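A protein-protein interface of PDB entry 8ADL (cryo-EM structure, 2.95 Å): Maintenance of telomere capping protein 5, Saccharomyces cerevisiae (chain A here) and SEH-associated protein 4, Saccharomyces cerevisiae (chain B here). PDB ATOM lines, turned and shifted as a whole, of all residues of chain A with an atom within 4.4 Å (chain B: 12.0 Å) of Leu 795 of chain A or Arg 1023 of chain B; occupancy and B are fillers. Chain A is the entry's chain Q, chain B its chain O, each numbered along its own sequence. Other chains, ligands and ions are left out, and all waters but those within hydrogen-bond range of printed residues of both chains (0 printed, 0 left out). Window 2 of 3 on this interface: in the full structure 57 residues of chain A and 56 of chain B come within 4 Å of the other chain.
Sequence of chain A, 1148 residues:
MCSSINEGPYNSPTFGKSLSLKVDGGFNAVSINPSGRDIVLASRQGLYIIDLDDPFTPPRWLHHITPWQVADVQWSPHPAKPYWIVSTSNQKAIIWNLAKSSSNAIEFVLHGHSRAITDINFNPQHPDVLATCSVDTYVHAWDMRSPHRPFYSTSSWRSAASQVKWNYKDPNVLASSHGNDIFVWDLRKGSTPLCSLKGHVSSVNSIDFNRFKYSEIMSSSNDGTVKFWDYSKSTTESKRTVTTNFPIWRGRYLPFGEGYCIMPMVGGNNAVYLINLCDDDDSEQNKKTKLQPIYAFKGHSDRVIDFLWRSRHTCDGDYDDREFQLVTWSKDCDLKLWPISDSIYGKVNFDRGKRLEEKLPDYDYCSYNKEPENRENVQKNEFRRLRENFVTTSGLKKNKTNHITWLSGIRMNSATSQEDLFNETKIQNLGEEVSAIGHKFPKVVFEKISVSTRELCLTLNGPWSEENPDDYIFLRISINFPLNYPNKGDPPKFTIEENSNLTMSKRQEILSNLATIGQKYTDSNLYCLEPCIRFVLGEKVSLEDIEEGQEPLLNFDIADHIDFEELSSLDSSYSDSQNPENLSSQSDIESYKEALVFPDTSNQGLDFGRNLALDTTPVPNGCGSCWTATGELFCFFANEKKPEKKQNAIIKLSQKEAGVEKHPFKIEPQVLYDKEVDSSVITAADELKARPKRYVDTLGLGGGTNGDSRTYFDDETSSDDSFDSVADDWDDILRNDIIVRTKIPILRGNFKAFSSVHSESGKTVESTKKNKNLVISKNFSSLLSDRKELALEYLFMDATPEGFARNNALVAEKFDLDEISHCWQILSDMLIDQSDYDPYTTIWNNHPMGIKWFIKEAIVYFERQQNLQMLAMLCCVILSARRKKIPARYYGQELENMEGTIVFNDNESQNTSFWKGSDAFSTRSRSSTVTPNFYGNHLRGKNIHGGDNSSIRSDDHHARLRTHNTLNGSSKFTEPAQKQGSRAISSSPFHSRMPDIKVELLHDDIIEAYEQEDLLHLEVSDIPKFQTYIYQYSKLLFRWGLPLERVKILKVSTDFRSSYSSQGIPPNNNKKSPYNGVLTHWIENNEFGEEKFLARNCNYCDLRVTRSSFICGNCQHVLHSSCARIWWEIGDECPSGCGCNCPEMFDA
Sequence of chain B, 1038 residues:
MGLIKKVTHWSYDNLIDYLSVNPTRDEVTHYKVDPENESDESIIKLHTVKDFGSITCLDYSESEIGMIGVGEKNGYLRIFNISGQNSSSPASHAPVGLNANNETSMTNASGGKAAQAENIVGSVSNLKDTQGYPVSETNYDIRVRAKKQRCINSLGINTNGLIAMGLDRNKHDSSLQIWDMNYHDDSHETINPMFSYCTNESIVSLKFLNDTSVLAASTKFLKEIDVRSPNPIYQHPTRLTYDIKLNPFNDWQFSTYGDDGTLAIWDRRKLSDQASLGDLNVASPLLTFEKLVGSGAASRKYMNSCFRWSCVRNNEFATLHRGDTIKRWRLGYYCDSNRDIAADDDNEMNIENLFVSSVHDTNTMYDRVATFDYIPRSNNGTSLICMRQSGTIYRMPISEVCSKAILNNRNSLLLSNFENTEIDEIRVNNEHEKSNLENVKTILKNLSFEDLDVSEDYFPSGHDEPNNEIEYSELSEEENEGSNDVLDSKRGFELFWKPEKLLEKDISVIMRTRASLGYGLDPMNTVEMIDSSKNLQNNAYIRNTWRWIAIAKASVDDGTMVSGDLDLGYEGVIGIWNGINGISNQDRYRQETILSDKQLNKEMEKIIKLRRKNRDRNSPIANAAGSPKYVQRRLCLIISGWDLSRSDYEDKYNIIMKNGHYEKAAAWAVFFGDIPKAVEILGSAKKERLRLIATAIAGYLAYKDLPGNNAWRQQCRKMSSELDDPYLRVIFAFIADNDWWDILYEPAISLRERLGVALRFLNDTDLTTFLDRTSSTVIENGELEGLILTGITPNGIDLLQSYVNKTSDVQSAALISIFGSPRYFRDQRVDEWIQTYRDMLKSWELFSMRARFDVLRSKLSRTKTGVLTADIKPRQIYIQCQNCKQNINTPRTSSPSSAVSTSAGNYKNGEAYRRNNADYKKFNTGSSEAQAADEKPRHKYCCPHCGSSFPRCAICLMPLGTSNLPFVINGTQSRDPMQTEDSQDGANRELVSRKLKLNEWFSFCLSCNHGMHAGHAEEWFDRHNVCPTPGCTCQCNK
The indole nitrogen (NE1) of Trp 1020 of chain B sits at hydrogen-bond distance from the backbone carbonyl oxygen (O) of Val 1026 of chain B (2.9 Å).
CD2 of Leu 795 of chain A touches NH2 of Arg 1023 of chain B (3.95 Å). Met 797 of chain A touches His 1024 of chain B. Arg 1023 of chain B touches Asp 798 of chain A (O to OD2, 3.6 Å). Trp 1020 of chain B touches Lys 1048 of chain A (CZ3 to CG, 3.7 Å). NH2 of Arg 1023 of chain B touches NZ of Lys 1048 of chain A, at 3.5 Å. Lys 1048 of chain A touches His 1024 of chain B.
Of chain B, only Arg 1023 comes within 4 Å of Leu 795 of chain A. No residue of chain B comes within 4 Å of Phe 796 of chain A. Met 797 of chain A touches just one residue of chain B: His 1024 (3.7 Å). Of chain B, only Arg 1023 (3.6 Å) comes within 4 Å of Asp 798 of chain A. No residue of chain B comes within 4 Å of Phe 804 of chain A. No residue of chain B comes within 4 Å of Asn 807 of chain A. Printed residues of chain B within 4 Å of Lys 1048 of chain A: Trp 1020, Arg 1023 and His 1024. Arg 1023 of chain B touches just these residues of chain A: Leu 795, Asp 798 and Lys 1048. Printed residues of chain A within 4 Å of His 1024 of chain B: Met 797 (3.7 Å) and Lys 1048 (3.4 Å). The nearest residue of chain B that does not touch Leu 795 of chain A is His 1024 of chain B (7.7 Å). The nearest printed residue of chain A that does not touch Arg 1023 of chain B is Tyr 794 of chain A (6.4 Å). The nearest printed residue of chain A that does not touch His 1024 of chain B is Asp 798 of chain A (4.3 Å).
Hydrophobic or aromatic side chains of chain B that line the printed part of chain A: Trp 1020 and His 1024. Among the printed residues, no Asp or Glu carboxylate lies within 4 Å of a Lys or Arg side-chain nitrogen of the other chain.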
ATOM      1  N   GLU A 793      16.521   7.159 -14.997  1.00  0.00           N
ATOM      2  CA  GLU A 793      16.783   8.044 -13.875  1.00  0.00           C
ATOM      3  C   GLU A 793      15.567   8.830 -13.405  1.00  0.00           C
ATOM      4  O   GLU A 793      15.621   9.409 -12.314  1.00  0.00           O
ATOM      5  CB  GLU A 793      17.914   9.024 -14.219  1.00  0.00           C
ATOM      6  CG  GLU A 793      19.251   8.358 -14.491  1.00  0.00           C
ATOM      7  CD  GLU A 793      20.412   9.329 -14.423  1.00  0.00           C
ATOM      8  OE1 GLU A 793      20.168  10.536 -14.211  1.00  0.00           O
ATOM      9  OE2 GLU A 793      21.569   8.887 -14.579  1.00  0.00           O
ATOM     10  N   TYR A 794      14.493   8.892 -14.190  1.00  0.00           N
ATOM     11  CA  TYR A 794      13.269   9.533 -13.727  1.00  0.00           C
ATOM     12  C   TYR A 794      12.641   8.750 -12.583  1.00  0.00           C
ATOM     13  O   TYR A 794      12.625   7.515 -12.582  1.00  0.00           O
ATOM     14  CB  TYR A 794      12.257   9.664 -14.868  1.00  0.00           C
ATOM     15  CG  TYR A 794      12.487  10.834 -15.797  1.00  0.00           C
ATOM     16  CD1 TYR A 794      13.335  11.876 -15.444  1.00  0.00           C
ATOM     17  CD2 TYR A 794      11.832  10.908 -17.019  1.00  0.00           C
ATOM     18  CE1 TYR A 794      13.537  12.950 -16.291  1.00  0.00           C
ATOM     19  CE2 TYR A 794      12.026  11.977 -17.871  1.00  0.00           C
ATOM     20  CZ  TYR A 794      12.879  12.994 -17.503  1.00  0.00           C
ATOM     21  OH  TYR A 794      13.074  14.060 -18.350  1.00  0.00           O
ATOM     22  N   LEU A 795      12.117   9.480 -11.602  1.00  0.00           N
ATOM     23  CA  LEU A 795      11.351   8.908 -10.505  1.00  0.00           C
ATOM     24  C   LEU A 795      10.049   9.679 -10.372  1.00  0.00           C
ATOM     25  O   LEU A 795      10.051  10.913 -10.412  1.00  0.00           O
ATOM     26  CB  LEU A 795      12.138   8.948  -9.192  1.00  0.00           C
ATOM     27  CG  LEU A 795      13.183   7.843  -9.018  1.00  0.00           C
ATOM     28  CD1 LEU A 795      13.848   7.937  -7.653  1.00  0.00           C
ATOM     29  CD2 LEU A 795      12.557   6.470  -9.224  1.00  0.00           C
ATOM     30  N   PHE A 796       8.939   8.955 -10.219  1.00  0.00           N
ATOM     31  CA  PHE A 796       7.641   9.607 -10.115  1.00  0.00           C
ATOM     32  C   PHE A 796       6.737   8.986  -9.055  1.00  0.00           C
ATOM     33  O   PHE A 796       5.562   9.368  -8.970  1.00  0.00           O
ATOM     34  CB  PHE A 796       6.923   9.611 -11.477  1.00  0.00           C
ATOM     35  CG  PHE A 796       6.921   8.278 -12.178  1.00  0.00           C
ATOM     36  CD1 PHE A 796       5.920   7.351 -11.931  1.00  0.00           C
ATOM     37  CD2 PHE A 796       7.906   7.961 -13.103  1.00  0.00           C
ATOM     38  CE1 PHE A 796       5.912   6.129 -12.577  1.00  0.00           C
ATOM     39  CE2 PHE A 796       7.904   6.742 -13.751  1.00  0.00           C
ATOM     40  CZ  PHE A 796       6.905   5.826 -13.489  1.00  0.00           C
ATOM     41  N   MET A 797       7.229   8.052  -8.250  1.00  0.00           N
ATOM     42  CA  MET A 797       6.374   7.469  -7.221  1.00  0.00           C
ATOM     43  C   MET A 797       6.994   7.480  -5.830  1.00  0.00           C
ATOM     44  O   MET A 797       6.287   7.737  -4.854  1.00  0.00           O
ATOM     45  CB  MET A 797       6.002   6.028  -7.611  1.00  0.00           C
ATOM     46  CG  MET A 797       4.864   5.437  -6.794  1.00  0.00           C
ATOM     47  SD  MET A 797       4.316   3.837  -7.417  1.00  0.00           S
ATOM     48  CE  MET A 797       3.944   4.250  -9.119  1.00  0.00           C
ATOM     49  N   ASP A 798       8.291   7.212  -5.713  1.00  0.00           N
ATOM     50  CA  ASP A 798       8.921   6.979  -4.411  1.00  0.00           C
ATOM     51  C   ASP A 798       9.613   8.240  -3.890  1.00  0.00           C
ATOM     52  O   ASP A 798      10.802   8.230  -3.562  1.00  0.00           O
ATOM     53  CB  ASP A 798       9.902   5.813  -4.507  1.00  0.00           C
ATOM     54  CG  ASP A 798       9.247   4.542  -5.011  1.00  0.00           C
ATOM     55  OD1 ASP A 798       8.008   4.528  -5.161  1.00  0.00           O
ATOM     56  OD2 ASP A 798       9.974   3.557  -5.260  1.00  0.00           O
ATOM     57  N   PHE A 804       9.558  14.385  -7.096  1.00  0.00           N
ATOM     58  CA  PHE A 804       9.569  13.866  -8.465  1.00  0.00           C
ATOM     59  C   PHE A 804      10.058  14.922  -9.444  1.00  0.00           C
ATOM     60  O   PHE A 804      10.963  14.673 -10.247  1.00  0.00           O
ATOM     61  CB  PHE A 804       8.174  13.406  -8.901  1.00  0.00           C
ATOM     62  CG  PHE A 804       7.427  12.584  -7.892  1.00  0.00           C
ATOM     63  CD1 PHE A 804       8.055  11.597  -7.150  1.00  0.00           C
ATOM     64  CD2 PHE A 804       6.065  12.780  -7.720  1.00  0.00           C
ATOM     65  CE1 PHE A 804       7.340  10.845  -6.243  1.00  0.00           C
ATOM     66  CE2 PHE A 804       5.349  12.029  -6.811  1.00  0.00           C
ATOM     67  CZ  PHE A 804       5.986  11.060  -6.072  1.00  0.00           C
ATOM     68  N   ASN A 807      13.766  15.916  -8.869  1.00  0.00           N
ATOM     69  CA  ASN A 807      14.653  14.871  -9.368  1.00  0.00           C
ATOM     70  C   ASN A 807      14.700  14.872 -10.890  1.00  0.00           C
ATOM     71  O   ASN A 807      15.776  14.724 -11.483  1.00  0.00           O
ATOM     72  CB  ASN A 807      14.202  13.507  -8.843  1.00  0.00           C
ATOM     73  CG  ASN A 807      15.074  12.371  -9.339  1.00  0.00           C
ATOM     74  OD1 ASN A 807      14.580  11.300  -9.688  1.00  0.00           O
ATOM     75  ND2 ASN A 807      16.384  12.597  -9.363  1.00  0.00           N
ATOM     76  N   ASN A 808      13.546  15.059 -11.538  1.00  0.00           N
ATOM     77  CA  ASN A 808      13.521  15.129 -12.996  1.00  0.00           C
ATOM     78  C   ASN A 808      14.228  16.376 -13.514  1.00  0.00           C
ATOM     79  O   ASN A 808      14.853  16.329 -14.579  1.00  0.00           O
ATOM     80  CB  ASN A 808      12.079  15.095 -13.498  1.00  0.00           C
ATOM     81  CG  ASN A 808      11.375  13.805 -13.153  1.00  0.00           C
ATOM     82  OD1 ASN A 808      11.995  12.847 -12.693  1.00  0.00           O
ATOM     83  ND2 ASN A 808      10.065  13.778 -13.356  1.00  0.00           N
ATOM     84  N   LYS A1048       4.466   0.573 -13.325  1.00  0.00           N
ATOM     85  CA  LYS A1048       4.232   1.722 -12.451  1.00  0.00           C
ATOM     86  C   LYS A1048       3.354   2.769 -13.131  1.00  0.00           C
ATOM     87  O   LYS A1048       2.383   3.265 -12.542  1.00  0.00           O
ATOM     88  CB  LYS A1048       5.565   2.344 -12.037  1.00  0.00           C
ATOM     89  CG  LYS A1048       6.414   1.483 -11.125  1.00  0.00           C
ATOM     90  CD  LYS A1048       7.768   2.132 -10.890  1.00  0.00           C
ATOM     91  CE  LYS A1048       8.903   1.193 -11.267  1.00  0.00           C
ATOM     92  NZ  LYS A1048      10.226   1.711 -10.821  1.00  0.00           N
ATOM     93  N   ILE B 955       4.781  -8.410 -15.424  1.00  0.00           N
ATOM     94  CA  ILE B 955       6.018  -7.694 -15.707  1.00  0.00           C
ATOM     95  C   ILE B 955       6.521  -8.038 -17.104  1.00  0.00           C
ATOM     96  O   ILE B 955       6.642  -7.157 -17.964  1.00  0.00           O
ATOM     97  CB  ILE B 955       7.087  -8.012 -14.646  1.00  0.00           C
ATOM     98  CG1 ILE B 955       6.506  -7.835 -13.244  1.00  0.00           C
ATOM     99  CG2 ILE B 955       8.301  -7.123 -14.828  1.00  0.00           C
ATOM    100  CD1 ILE B 955       6.038  -6.433 -12.943  1.00  0.00           C
ATOM    101  N   MET B1012       2.733 -13.597 -10.482  1.00  0.00           N
ATOM    102  CA  MET B1012       3.968 -13.147 -11.104  1.00  0.00           C
ATOM    103  C   MET B1012       5.029 -14.211 -10.876  1.00  0.00           C
ATOM    104  O   MET B1012       4.943 -14.989  -9.925  1.00  0.00           O
ATOM    105  CB  MET B1012       4.474 -11.831 -10.500  1.00  0.00           C
ATOM    106  CG  MET B1012       3.425 -10.781 -10.236  1.00  0.00           C
ATOM    107  SD  MET B1012       4.030  -9.662  -8.966  1.00  0.00           S
ATOM    108  CE  MET B1012       5.298  -8.797  -9.879  1.00  0.00           C
ATOM    109  N   ALA B1014       8.548 -15.522  -9.493  1.00  0.00           N
ATOM    110  CA  ALA B1014       9.102 -15.241  -8.171  1.00  0.00           C
ATOM    111  C   ALA B1014      10.253 -14.249  -8.237  1.00  0.00           C
ATOM    112  O   ALA B1014      10.404 -13.409  -7.343  1.00  0.00           O
ATOM    113  CB  ALA B1014       9.553 -16.535  -7.503  1.00  0.00           C
ATOM    114  N   GLY B1015      11.081 -14.335  -9.279  1.00  0.00           N
ATOM    115  CA  GLY B1015      12.101 -13.320  -9.477  1.00  0.00           C
ATOM    116  C   GLY B1015      11.495 -11.968  -9.797  1.00  0.00           C
ATOM    117  O   GLY B1015      11.933 -10.939  -9.272  1.00  0.00           O
ATOM    118  N   HIS B1016      10.455 -11.959 -10.637  1.00  0.00           N
ATOM    119  CA  HIS B1016       9.745 -10.724 -10.945  1.00  0.00           C
ATOM    120  C   HIS B1016       9.031 -10.176  -9.717  1.00  0.00           C
ATOM    121  O   HIS B1016       9.016  -8.960  -9.493  1.00  0.00           O
ATOM    122  CB  HIS B1016       8.743 -10.962 -12.073  1.00  0.00           C
ATOM    123  CG  HIS B1016       9.363 -11.453 -13.344  1.00  0.00           C
ATOM    124  ND1 HIS B1016       8.621 -12.011 -14.362  1.00  0.00           N
ATOM    125  CD2 HIS B1016      10.649 -11.462 -13.767  1.00  0.00           C
ATOM    126  CE1 HIS B1016       9.424 -12.352 -15.353  1.00  0.00           C
ATOM    127  NE2 HIS B1016      10.660 -12.027 -15.019  1.00  0.00           N
ATOM    128  N   ALA B1017       8.442 -11.060  -8.906  1.00  0.00           N
ATOM    129  CA  ALA B1017       7.760 -10.621  -7.693  1.00  0.00           C
ATOM    130  C   ALA B1017       8.742 -10.063  -6.672  1.00  0.00           C
ATOM    131  O   ALA B1017       8.432  -9.088  -5.979  1.00  0.00           O
ATOM    132  CB  ALA B1017       6.957 -11.773  -7.090  1.00  0.00           C
ATOM    133  N   GLU B1018       9.926 -10.668  -6.558  1.00  0.00           N
ATOM    134  CA  GLU B1018      10.941 -10.133  -5.658  1.00  0.00           C
ATOM    135  C   GLU B1018      11.468  -8.792  -6.153  1.00  0.00           C
ATOM    136  O   GLU B1018      11.696  -7.877  -5.353  1.00  0.00           O
ATOM    137  CB  GLU B1018      12.086 -11.134  -5.503  1.00  0.00           C
ATOM    138  CG  GLU B1018      13.203 -10.666  -4.582  1.00  0.00           C
ATOM    139  CD  GLU B1018      14.498 -11.422  -4.799  1.00  0.00           C
ATOM    140  OE1 GLU B1018      14.545 -12.269  -5.714  1.00  0.00           O
ATOM    141  OE2 GLU B1018      15.469 -11.165  -4.058  1.00  0.00           O
ATOM    142  N   GLU B1019      11.661  -8.652  -7.469  1.00  0.00           N
ATOM    143  CA  GLU B1019      12.157  -7.391  -8.014  1.00  0.00           C
ATOM    144  C   GLU B1019      11.121  -6.276  -7.916  1.00  0.00           C
ATOM    145  O   GLU B1019      11.486  -5.108  -7.744  1.00  0.00           O
ATOM    146  CB  GLU B1019      12.594  -7.587  -9.466  1.00  0.00           C
ATOM    147  CG  GLU B1019      13.601  -6.560  -9.952  1.00  0.00           C
ATOM    148  CD  GLU B1019      14.068  -6.829 -11.369  1.00  0.00           C
ATOM    149  OE1 GLU B1019      13.574  -7.798 -11.984  1.00  0.00           O
ATOM    150  OE2 GLU B1019      14.929  -6.074 -11.866  1.00  0.00           O
ATOM    151  N   TRP B1020       9.833  -6.611  -8.021  1.00  0.00           N
ATOM    152  CA  TRP B1020       8.780  -5.604  -7.953  1.00  0.00           C
ATOM    153  C   TRP B1020       8.445  -5.232  -6.513  1.00  0.00           C
ATOM    154  O   TRP B1020       8.373  -4.047  -6.171  1.00  0.00           O
ATOM    155  CB  TRP B1020       7.536  -6.114  -8.679  1.00  0.00           C
ATOM    156  CG  TRP B1020       6.285  -5.340  -8.402  1.00  0.00           C
ATOM    157  CD1 TRP B1020       5.272  -5.701  -7.564  1.00  0.00           C
ATOM    158  CD2 TRP B1020       5.899  -4.088  -8.980  1.00  0.00           C
ATOM    159  NE1 TRP B1020       4.285  -4.747  -7.574  1.00  0.00           N
ATOM    160  CE2 TRP B1020       4.645  -3.746  -8.436  1.00  0.00           C
ATOM    161  CE3 TRP B1020       6.494  -3.220  -9.898  1.00  0.00           C
ATOM    162  CZ2 TRP B1020       3.977  -2.576  -8.780  1.00  0.00           C
ATOM    163  CZ3 TRP B1020       5.828  -2.059 -10.240  1.00  0.00           C
ATOM    164  CH2 TRP B1020       4.583  -1.747  -9.681  1.00  0.00           C
ATOM    165  N   PHE B1021       8.235  -6.231  -5.655  1.00  0.00           N
ATOM    166  CA  PHE B1021       7.783  -5.994  -4.291  1.00  0.00           C
ATOM    167  C   PHE B1021       8.891  -5.516  -3.363  1.00  0.00           C
ATOM    168  O   PHE B1021       8.606  -5.184  -2.208  1.00  0.00           O
ATOM    169  CB  PHE B1021       7.143  -7.264  -3.730  1.00  0.00           C
ATOM    170  CG  PHE B1021       5.724  -7.468  -4.175  1.00  0.00           C
ATOM    171  CD1 PHE B1021       4.747  -6.541  -3.859  1.00  0.00           C
ATOM    172  CD2 PHE B1021       5.370  -8.581  -4.917  1.00  0.00           C
ATOM    173  CE1 PHE B1021       3.440  -6.724  -4.269  1.00  0.00           C
ATOM    174  CE2 PHE B1021       4.065  -8.770  -5.330  1.00  0.00           C
ATOM    175  CZ  PHE B1021       3.100  -7.840  -5.006  1.00  0.00           C
ATOM    176  N   ASP B1022      10.144  -5.493  -3.825  1.00  0.00           N
ATOM    177  CA  ASP B1022      11.216  -4.916  -3.022  1.00  0.00           C
ATOM    178  C   ASP B1022      11.054  -3.408  -2.890  1.00  0.00           C
ATOM    179  O   ASP B1022      11.283  -2.844  -1.813  1.00  0.00           O
ATOM    180  CB  ASP B1022      12.575  -5.255  -3.631  1.00  0.00           C
ATOM    181  CG  ASP B1022      13.731  -4.777  -2.776  1.00  0.00           C
ATOM    182  OD1 ASP B1022      14.035  -5.439  -1.763  1.00  0.00           O
ATOM    183  OD2 ASP B1022      14.337  -3.739  -3.117  1.00  0.00           O
ATOM    184  N   ARG B1023      10.660  -2.738  -3.971  1.00  0.00           N
ATOM    185  CA  ARG B1023      10.517  -1.289  -3.994  1.00  0.00           C
ATOM    186  C   ARG B1023       9.064  -0.841  -4.090  1.00  0.00           C
ATOM    187  O   ARG B1023       8.806   0.355  -4.258  1.00  0.00           O
ATOM    188  CB  ARG B1023      11.326  -0.699  -5.152  1.00  0.00           C
ATOM    189  CG  ARG B1023      11.174  -1.455  -6.459  1.00  0.00           C
ATOM    190  CD  ARG B1023      12.111  -0.911  -7.525  1.00  0.00           C
ATOM    191  NE  ARG B1023      12.032   0.541  -7.633  1.00  0.00           N
ATOM    192  CZ  ARG B1023      12.810   1.278  -8.413  1.00  0.00           C
ATOM    193  NH1 ARG B1023      13.745   0.730  -9.173  1.00  0.00           N
ATOM    194  NH2 ARG B1023      12.649   2.598  -8.430  1.00  0.00           N
ATOM    195  N   HIS B1024       8.111  -1.765  -3.992  1.00  0.00           N
ATOM    196  CA  HIS B1024       6.698  -1.424  -4.060  1.00  0.00           C
ATOM    197  C   HIS B1024       5.916  -2.328  -3.119  1.00  0.00           C
ATOM    198  O   HIS B1024       6.412  -3.356  -2.656  1.00  0.00           O
ATOM    199  CB  HIS B1024       6.149  -1.554  -5.485  1.00  0.00           C
ATOM    200  CG  HIS B1024       6.681  -0.524  -6.432  1.00  0.00           C
ATOM    201  ND1 HIS B1024       7.881  -0.672  -7.091  1.00  0.00           N
ATOM    202  CD2 HIS B1024       6.181   0.671  -6.822  1.00  0.00           C
ATOM    203  CE1 HIS B1024       8.096   0.387  -7.850  1.00  0.00           C
ATOM    204  NE2 HIS B1024       7.079   1.217  -7.705  1.00  0.00           N
ATOM    205  N   ASN B1025       4.675  -1.924  -2.837  1.00  0.00           N
ATOM    206  CA  ASN B1025       3.855  -2.653  -1.878  1.00  0.00           C
ATOM    207  C   ASN B1025       2.414  -2.823  -2.349  1.00  0.00           C
ATOM    208  O   ASN B1025       1.520  -3.004  -1.515  1.00  0.00           O
ATOM    209  CB  ASN B1025       3.865  -1.953  -0.516  1.00  0.00           C
ATOM    210  CG  ASN B1025       5.123  -2.243   0.276  1.00  0.00           C
ATOM    211  OD1 ASN B1025       5.618  -3.370   0.283  1.00  0.00           O
ATOM    212  ND2 ASN B1025       5.647  -1.225   0.948  1.00  0.00           N
ATOM    213  N   VAL B1026       2.160  -2.766  -3.657  1.00  0.00           N
ATOM    214  CA  VAL B1026       0.819  -2.942  -4.194  1.00  0.00           C
ATOM    215  C   VAL B1026       0.887  -3.985  -5.304  1.00  0.00           C
ATOM    216  O   VAL B1026       1.950  -4.255  -5.869  1.00  0.00           O
ATOM    217  CB  VAL B1026       0.229  -1.600  -4.704  1.00  0.00           C
ATOM    218  CG1 VAL B1026       0.835  -1.197  -6.047  1.00  0.00           C
ATOM    219  CG2 VAL B1026      -1.303  -1.623  -4.744  1.00  0.00           C
ATOM    220  N   CYS B1027      -0.257  -4.612  -5.572  1.00  0.00           N
ATOM    221  CA  CYS B1027      -0.347  -5.597  -6.645  1.00  0.00           C
ATOM    222  C   CYS B1027      -0.125  -4.916  -7.991  1.00  0.00           C
ATOM    223  O   CYS B1027      -0.741  -3.879  -8.263  1.00  0.00           O
ATOM    224  CB  CYS B1027      -1.707  -6.288  -6.618  1.00  0.00           C
ATOM    225  SG  CYS B1027      -1.923  -7.595  -7.843  1.00  0.00           S
ATOM    226  N   PRO B1028       0.740  -5.458  -8.853  1.00  0.00           N
ATOM    227  CA  PRO B1028       1.073  -4.757 -10.103  1.00  0.00           C
ATOM    228  C   PRO B1028      -0.026  -4.789 -11.154  1.00  0.00           C
ATOM    229  O   PRO B1028       0.085  -4.067 -12.152  1.00  0.00           O
ATOM    230  CB  PRO B1028       2.315  -5.509 -10.587  1.00  0.00           C
ATOM    231  CG  PRO B1028       2.111  -6.873 -10.081  1.00  0.00           C
ATOM    232  CD  PRO B1028       1.500  -6.710  -8.718  1.00  0.00           C
ATOM    233  N   CYS B1034      -3.952  -4.678  -3.125  1.00  0.00           N
ATOM    234  CA  CYS B1034      -3.683  -5.797  -2.225  1.00  0.00           C
ATOM    235  C   CYS B1034      -2.181  -5.852  -1.985  1.00  0.00           C
ATOM    236  O   CYS B1034      -1.420  -6.170  -2.902  1.00  0.00           O
ATOM    237  CB  CYS B1034      -4.196  -7.109  -2.811  1.00  0.00           C
ATOM    238  SG  CYS B1034      -3.706  -8.586  -1.894  1.00  0.00           S
ATOM    239  N   GLN B1035      -1.759  -5.543  -0.763  1.00  0.00           N
ATOM    240  CA  GLN B1035      -0.341  -5.561  -0.404  1.00  0.00           C
ATOM    241  C   GLN B1035       0.071  -7.008  -0.175  1.00  0.00           C
ATOM    242  O   GLN B1035      -0.067  -7.554   0.920  1.00  0.00           O
ATOM    243  CB  GLN B1035      -0.087  -4.705   0.829  1.00  0.00           C
ATOM    244  CG  GLN B1035      -0.862  -3.400   0.848  1.00  0.00           C
ATOM    245  CD  GLN B1035      -0.394  -2.461   1.941  1.00  0.00           C
ATOM    246  OE1 GLN B1035       0.508  -2.789   2.712  1.00  0.00           O
ATOM    247  NE2 GLN B1035      -1.006  -1.285   2.015  1.00  0.00           N
ATOM    248  N   CYS B1036       0.595  -7.637  -1.228  1.00  0.00           N
ATOM    249  CA  CYS B1036       0.967  -9.044  -1.170  1.00  0.00           C
ATOM    250  C   CYS B1036       2.296  -9.291  -0.468  1.00  0.00           C
ATOM    251  O   CYS B1036       2.623 -10.451  -0.196  1.00  0.00           O
ATOM    252  CB  CYS B1036       1.027  -9.627  -2.584  1.00  0.00           C
ATOM    253  SG  CYS B1036      -0.373  -9.197  -3.637  1.00  0.00           S
ATOM    254  N   ASN B1037       3.061  -8.251  -0.165  1.00  0.00           N
ATOM    255  CA  ASN B1037       4.343  -8.432   0.502  1.00  0.00           C
ATOM    256  C   ASN B1037       4.531  -7.367   1.580  1.00  0.00           C
ATOM    257  O   ASN B1037       4.113  -7.549   2.724  1.00  0.00           O
ATOM    258  CB  ASN B1037       5.488  -8.380  -0.515  1.00  0.00           C
ATOM    259  CG  ASN B1037       6.803  -8.888   0.050  1.00  0.00           C
ATOM    260  OD1 ASN B1037       6.877  -9.321   1.200  1.00  0.00           O
ATOM    261  ND2 ASN B1037       7.850  -8.842  -0.764  1.00  0.00           N
